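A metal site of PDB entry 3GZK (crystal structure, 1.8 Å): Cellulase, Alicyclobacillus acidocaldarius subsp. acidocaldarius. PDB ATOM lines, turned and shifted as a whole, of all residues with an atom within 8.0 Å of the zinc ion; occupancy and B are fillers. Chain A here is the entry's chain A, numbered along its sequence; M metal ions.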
ATOM      1  N   GLN A 102     -14.269 -14.971 -12.648  1.00  0.00           N
ATOM      2  CA  GLN A 102     -13.227 -15.091 -13.670  1.00  0.00           C
ATOM      3  C   GLN A 102     -13.712 -15.778 -14.955  1.00  0.00           C
ATOM      4  O   GLN A 102     -12.941 -15.925 -15.900  1.00  0.00           O
ATOM      5  CB  GLN A 102     -12.030 -15.877 -13.118  1.00  0.00           C
ATOM      6  CG  GLN A 102     -11.272 -15.227 -11.975  1.00  0.00           C
ATOM      7  CD  GLN A 102     -10.522 -13.982 -12.395  1.00  0.00           C
ATOM      8  OE1 GLN A 102     -11.022 -12.881 -12.237  1.00  0.00           O
ATOM      9  NE2 GLN A 102      -9.321 -14.148 -12.950  1.00  0.00           N
ATOM     10  N   LEU A 103     -14.965 -16.220 -14.998  1.00  0.00           N
ATOM     11  CA  LEU A 103     -15.448 -16.981 -16.153  1.00  0.00           C
ATOM     12  C   LEU A 103     -15.304 -16.193 -17.460  1.00  0.00           C
ATOM     13  O   LEU A 103     -15.576 -14.987 -17.507  1.00  0.00           O
ATOM     14  CB  LEU A 103     -16.893 -17.462 -15.965  1.00  0.00           C
ATOM     15  CG  LEU A 103     -17.057 -18.683 -15.060  1.00  0.00           C
ATOM     16  CD1 LEU A 103     -18.498 -18.840 -14.632  1.00  0.00           C
ATOM     17  CD2 LEU A 103     -16.556 -19.944 -15.739  1.00  0.00           C
ATOM     18  N   CYS A 104     -14.861 -16.884 -18.504  1.00  0.00           N
ATOM     19  CA  CYS A 104     -14.642 -16.318 -19.816  1.00  0.00           C
ATOM     20  C   CYS A 104     -15.628 -16.921 -20.819  1.00  0.00           C
ATOM     21  O   CYS A 104     -15.896 -18.119 -20.796  1.00  0.00           O
ATOM     22  CB  CYS A 104     -13.201 -16.612 -20.250  1.00  0.00           C
ATOM     23  SG  CYS A 104     -12.699 -15.923 -21.826  1.00  0.00           S
ATOM     24  N   GLY A 105     -16.173 -16.081 -21.699  1.00  0.00           N
ATOM     25  CA  GLY A 105     -17.107 -16.548 -22.731  1.00  0.00           C
ATOM     26  C   GLY A 105     -18.481 -16.940 -22.214  1.00  0.00           C
ATOM     27  O   GLY A 105     -19.197 -17.675 -22.885  1.00  0.00           O
ATOM     28  N   VAL A 106     -18.850 -16.467 -21.024  1.00  0.00           N
ATOM     29  CA  VAL A 106     -20.162 -16.754 -20.438  1.00  0.00           C
ATOM     30  C   VAL A 106     -20.766 -15.471 -19.874  1.00  0.00           C
ATOM     31  O   VAL A 106     -20.081 -14.648 -19.251  1.00  0.00           O
ATOM     32  CB  VAL A 106     -20.105 -17.865 -19.332  1.00  0.00           C
ATOM     33  CG1 VAL A 106     -18.998 -18.885 -19.612  1.00  0.00           C
ATOM     34  CG2 VAL A 106     -19.904 -17.280 -17.956  1.00  0.00           C
ATOM     35  N   HIS A 118     -21.294  -8.923 -16.672  1.00  0.00           N
ATOM     36  CA  HIS A 118     -20.908  -8.607 -18.031  1.00  0.00           C
ATOM     37  C   HIS A 118     -21.331  -9.692 -19.011  1.00  0.00           C
ATOM     38  O   HIS A 118     -21.626 -10.836 -18.632  1.00  0.00           O
ATOM     39  CB  HIS A 118     -19.405  -8.323 -18.143  1.00  0.00           C
ATOM     40  CG  HIS A 118     -18.520  -9.500 -17.854  1.00  0.00           C
ATOM     41  ND1 HIS A 118     -18.256 -10.472 -18.791  1.00  0.00           N
ATOM     42  CD2 HIS A 118     -17.815  -9.840 -16.747  1.00  0.00           C
ATOM     43  CE1 HIS A 118     -17.433 -11.372 -18.272  1.00  0.00           C
ATOM     44  NE2 HIS A 118     -17.160 -11.009 -17.023  1.00  0.00           N
ATOM     45  N   GLY A 119     -21.391  -9.314 -20.288  1.00  0.00           N
ATOM     46  CA  GLY A 119     -21.723 -10.239 -21.359  1.00  0.00           C
ATOM     47  C   GLY A 119     -20.519 -11.100 -21.700  1.00  0.00           C
ATOM     48  O   GLY A 119     -19.391 -10.790 -21.287  1.00  0.00           O
ATOM     49  N   ALA A 120     -20.756 -12.158 -22.467  1.00  0.00           N
ATOM     50  CA  ALA A 120     -19.722 -13.132 -22.803  1.00  0.00           C
ATOM     51  C   ALA A 120     -18.528 -12.462 -23.484  1.00  0.00           C
ATOM     52  O   ALA A 120     -18.707 -11.704 -24.441  1.00  0.00           O
ATOM     53  CB  ALA A 120     -20.278 -14.230 -23.683  1.00  0.00           C
ATOM     54  N   CYS A 121     -17.325 -12.728 -22.976  1.00  0.00           N
ATOM     55  CA  CYS A 121     -16.087 -12.141 -23.480  1.00  0.00           C
ATOM     56  C   CYS A 121     -15.237 -13.168 -24.226  1.00  0.00           C
ATOM     57  O   CYS A 121     -15.394 -14.373 -24.046  1.00  0.00           O
ATOM     58  CB  CYS A 121     -15.275 -11.558 -22.331  1.00  0.00           C
ATOM     59  SG  CYS A 121     -14.996 -12.763 -20.988  1.00  0.00           S
ATOM     60  N   HIS A 122     -14.327 -12.655 -25.063  1.00  0.00           N
ATOM     61  CA  HIS A 122     -13.379 -13.454 -25.827  1.00  0.00           C
ATOM     62  C   HIS A 122     -14.045 -14.615 -26.586  1.00  0.00           C
ATOM     63  O   HIS A 122     -13.569 -15.741 -26.558  1.00  0.00           O
ATOM     64  CB  HIS A 122     -12.264 -13.963 -24.904  1.00  0.00           C
ATOM     65  CG  HIS A 122     -11.589 -12.877 -24.137  1.00  0.00           C
ATOM     66  ND1 HIS A 122     -11.894 -12.600 -22.828  1.00  0.00           N
ATOM     67  CD2 HIS A 122     -10.625 -11.993 -24.489  1.00  0.00           C
ATOM     68  CE1 HIS A 122     -11.156 -11.584 -22.404  1.00  0.00           C
ATOM     69  NE2 HIS A 122     -10.383 -11.197 -23.409  1.00  0.00           N
ATOM     70  N   THR A 123     -15.132 -14.307 -27.299  1.00  0.00           N
ATOM     71  CA  THR A 123     -15.922 -15.338 -27.971  1.00  0.00           C
ATOM     72  C   THR A 123     -15.381 -15.784 -29.342  1.00  0.00           C
ATOM     73  O   THR A 123     -15.858 -16.767 -29.910  1.00  0.00           O
ATOM     74  CB  THR A 123     -17.410 -14.911 -28.093  1.00  0.00           C
ATOM     75  OG1 THR A 123     -17.499 -13.569 -28.617  1.00  0.00           O
ATOM     76  CG2 THR A 123     -18.065 -14.949 -26.729  1.00  0.00           C
ATOM     77  N   GLY A 139     -14.649 -20.628 -22.792  1.00  0.00           N
ATOM     78  CA  GLY A 139     -14.972 -21.013 -21.425  1.00  0.00           C
ATOM     79  C   GLY A 139     -13.792 -20.986 -20.484  1.00  0.00           C
ATOM     80  O   GLY A 139     -12.742 -20.442 -20.798  1.00  0.00           O
ATOM     81  N   GLY A 140     -13.986 -21.577 -19.317  1.00  0.00           N
ATOM     82  CA  GLY A 140     -12.933 -21.590 -18.308  1.00  0.00           C
ATOM     83  C   GLY A 140     -12.713 -20.226 -17.688  1.00  0.00           C
ATOM     84  O   GLY A 140     -13.595 -19.351 -17.725  1.00  0.00           O
ATOM     85  N   TRP A 141     -11.529 -20.040 -17.113  1.00  0.00           N
ATOM     86  CA  TRP A 141     -11.253 -18.878 -16.273  1.00  0.00           C
ATOM     87  C   TRP A 141     -10.147 -18.004 -16.821  1.00  0.00           C
ATOM     88  O   TRP A 141      -9.093 -18.501 -17.231  1.00  0.00           O
ATOM     89  CB  TRP A 141     -10.802 -19.331 -14.870  1.00  0.00           C
ATOM     90  CG  TRP A 141     -11.773 -20.214 -14.183  1.00  0.00           C
ATOM     91  CD1 TRP A 141     -13.126 -20.099 -14.186  1.00  0.00           C
ATOM     92  CD2 TRP A 141     -11.461 -21.359 -13.372  1.00  0.00           C
ATOM     93  NE1 TRP A 141     -13.692 -21.102 -13.417  1.00  0.00           N
ATOM     94  CE2 TRP A 141     -12.686 -21.879 -12.903  1.00  0.00           C
ATOM     95  CE3 TRP A 141     -10.279 -21.981 -12.974  1.00  0.00           C
ATOM     96  CZ2 TRP A 141     -12.762 -23.005 -12.062  1.00  0.00           C
ATOM     97  CZ3 TRP A 141     -10.343 -23.104 -12.139  1.00  0.00           C
ATOM     98  CH2 TRP A 141     -11.578 -23.600 -11.694  1.00  0.00           C
ATOM     99  N   HIS A 142     -10.367 -16.703 -16.756  1.00  0.00           N
ATOM    100  CA  HIS A 142      -9.267 -15.752 -16.841  1.00  0.00           C
ATOM    101  C   HIS A 142      -8.295 -16.095 -15.701  1.00  0.00           C
ATOM    102  O   HIS A 142      -8.695 -16.318 -14.568  1.00  0.00           O
ATOM    103  CB  HIS A 142      -9.768 -14.319 -16.680  1.00  0.00           C
ATOM    104  CG  HIS A 142     -10.781 -13.905 -17.695  1.00  0.00           C
ATOM    105  ND1 HIS A 142     -11.871 -13.130 -17.368  1.00  0.00           N
ATOM    106  CD2 HIS A 142     -10.875 -14.126 -19.030  1.00  0.00           C
ATOM    107  CE1 HIS A 142     -12.598 -12.891 -18.446  1.00  0.00           C
ATOM    108  NE2 HIS A 142     -12.017 -13.497 -19.474  1.00  0.00           N
ATOM    109  N   ASP A 146      -5.134 -10.499 -15.674  1.00  0.00           N
ATOM    110  CA  ASP A 146      -5.276 -10.464 -17.126  1.00  0.00           C
ATOM    111  C   ASP A 146      -6.369 -11.430 -17.604  1.00  0.00           C
ATOM    112  O   ASP A 146      -7.098 -12.020 -16.789  1.00  0.00           O
ATOM    113  CB  ASP A 146      -3.932 -10.818 -17.794  1.00  0.00           C
ATOM    114  CG  ASP A 146      -3.615 -12.322 -17.705  1.00  0.00           C
ATOM    115  OD1 ASP A 146      -3.761 -12.849 -16.589  1.00  0.00           O
ATOM    116  OD2 ASP A 146      -3.242 -12.955 -18.728  1.00  0.00           O
ATOM    117  N   TYR A 147      -6.475 -11.603 -18.917  1.00  0.00           N
ATOM    118  CA  TYR A 147      -7.531 -12.417 -19.499  1.00  0.00           C
ATOM    119  C   TYR A 147      -7.048 -13.653 -20.219  1.00  0.00           C
ATOM    120  O   TYR A 147      -7.835 -14.357 -20.852  1.00  0.00           O
ATOM    121  CB  TYR A 147      -8.410 -11.556 -20.422  1.00  0.00           C
ATOM    122  CG  TYR A 147      -9.068 -10.396 -19.723  1.00  0.00           C
ATOM    123  CD1 TYR A 147      -9.793 -10.595 -18.545  1.00  0.00           C
ATOM    124  CD2 TYR A 147      -8.972  -9.091 -20.222  1.00  0.00           C
ATOM    125  CE1 TYR A 147     -10.410  -9.539 -17.902  1.00  0.00           C
ATOM    126  CE2 TYR A 147      -9.589  -8.026 -19.558  1.00  0.00           C
ATOM    127  CZ  TYR A 147     -10.300  -8.260 -18.404  1.00  0.00           C
ATOM    128  OH  TYR A 147     -10.927  -7.229 -17.731  1.00  0.00           O
ATOM    129  N   GLY A 148      -5.750 -13.944 -20.112  1.00  0.00           N
ATOM    130  CA  GLY A 148      -5.204 -15.174 -20.682  1.00  0.00           C
ATOM    131  C   GLY A 148      -5.713 -16.410 -19.961  1.00  0.00           C
ATOM    132  O   GLY A 148      -6.079 -16.346 -18.794  1.00  0.00           O
ATOM    133  N   LYS A 149      -5.744 -17.525 -20.668  1.00  0.00           N
ATOM    134  CA  LYS A 149      -6.109 -18.804 -20.076  1.00  0.00           C
ATOM    135  C   LYS A 149      -4.955 -19.744 -20.379  1.00  0.00           C
ATOM    136  O   LYS A 149      -4.637 -20.016 -21.545  1.00  0.00           O
ATOM    137  CB  LYS A 149      -7.440 -19.315 -20.636  1.00  0.00           C
ATOM    138  CG  LYS A 149      -8.546 -18.255 -20.647  1.00  0.00           C
ATOM    139  CD  LYS A 149      -9.935 -18.820 -20.922  1.00  0.00           C
ATOM    140  CE  LYS A 149     -10.098 -19.264 -22.358  1.00  0.00           C
ATOM    141  NZ  LYS A 149     -11.548 -19.275 -22.796  1.00  0.00           N
ATOM    142  N   PRO A 228     -13.536  -6.944 -19.621  1.00  0.00           N
ATOM    143  CA  PRO A 228     -13.362  -8.230 -20.337  1.00  0.00           C
ATOM    144  C   PRO A 228     -14.025  -8.259 -21.716  1.00  0.00           C
ATOM    145  O   PRO A 228     -13.415  -8.692 -22.687  1.00  0.00           O
ATOM    146  CB  PRO A 228     -14.011  -9.257 -19.403  1.00  0.00           C
ATOM    147  CG  PRO A 228     -14.756  -8.485 -18.368  1.00  0.00           C
ATOM    148  CD  PRO A 228     -14.150  -7.122 -18.302  1.00  0.00           C
ATOM    149  N   GLU A 229     -15.269  -7.789 -21.778  1.00  0.00           N
ATOM    150  CA  GLU A 229     -16.034  -7.772 -23.024  1.00  0.00           C
ATOM    151  C   GLU A 229     -15.520  -6.757 -24.059  1.00  0.00           C
ATOM    152  O   GLU A 229     -15.868  -6.865 -25.235  1.00  0.00           O
ATOM    153  CB  GLU A 229     -17.533  -7.545 -22.748  1.00  0.00           C
ATOM    154  CG  GLU A 229     -17.908  -6.147 -22.232  1.00  0.00           C
ATOM    155  CD  GLU A 229     -17.762  -5.989 -20.727  1.00  0.00           C
ATOM    156  OE1 GLU A 229     -16.925  -6.673 -20.107  1.00  0.00           O
ATOM    157  OE2 GLU A 229     -18.492  -5.148 -20.155  1.00  0.00           O
ATOM    158  N   ASP A 231     -12.249  -6.361 -24.620  1.00  0.00           N
ATOM    159  CA  ASP A 231     -10.949  -6.858 -25.057  1.00  0.00           C
ATOM    160  C   ASP A 231     -11.139  -7.682 -26.329  1.00  0.00           C
ATOM    161  O   ASP A 231     -11.443  -8.873 -26.261  1.00  0.00           O
ATOM    162  CB  ASP A 231     -10.300  -7.691 -23.944  1.00  0.00           C
ATOM    163  CG  ASP A 231      -8.963  -8.300 -24.351  1.00  0.00           C
ATOM    164  OD1 ASP A 231      -8.288  -7.766 -25.261  1.00  0.00           O
ATOM    165  OD2 ASP A 231      -8.588  -9.329 -23.745  1.00  0.00           O
ATOM    166  N   LEU A 235      -7.217 -13.691 -30.643  1.00  0.00           N
ATOM    167  CA  LEU A 235      -6.743 -14.722 -29.716  1.00  0.00           C
ATOM    168  C   LEU A 235      -5.801 -15.672 -30.445  1.00  0.00           C
ATOM    169  O   LEU A 235      -6.053 -16.057 -31.596  1.00  0.00           O
ATOM    170  CB  LEU A 235      -7.914 -15.525 -29.162  1.00  0.00           C
ATOM    171  CG  LEU A 235      -8.832 -14.773 -28.195  1.00  0.00           C
ATOM    172  CD1 LEU A 235     -10.078 -15.596 -27.941  1.00  0.00           C
ATOM    173  CD2 LEU A 235      -8.104 -14.472 -26.878  1.00  0.00           C
HETATM  174 ZN    ZN M   1     -12.923 -13.724 -21.365  1.00  0.00          ZN
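O of Cys 121 sits at hydrogen-bond distance from N of Gly 105, at 3.0 Å.
The side-chain amino group (NZ) of Lys 149 sits close to the side-chain sulfur (SG) of Cys 104, 3.7 Å away.
OD2 of Asp 231 is in hydrogen-bond range of NE2 of His 122, at 2.6 Å.
O of Gly 140 sits at hydrogen-bond distance from N of Cys 104.
O of Cys 104 sits close to N of Gly 139, 3.4 Å away.
O of His 142 is in hydrogen-bond range of NE2 of Gln 102, at 2.8 Å.
The nearest printed residue that does not touch the zinc ion is Gly 105 (4.03 Å).
The zinc ion is bound by NE2 of His 142, 2.1 Å away.
The zinc ion is bound by ND1 of His 122, 2.1 Å away.
SG of Cys 104 is bound to the zinc ion, 2.3 Å away.
The zinc ion is bound by SG of Cys 121, at 2.3 Å.
The zinc ion has four donor atoms within binding distance.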
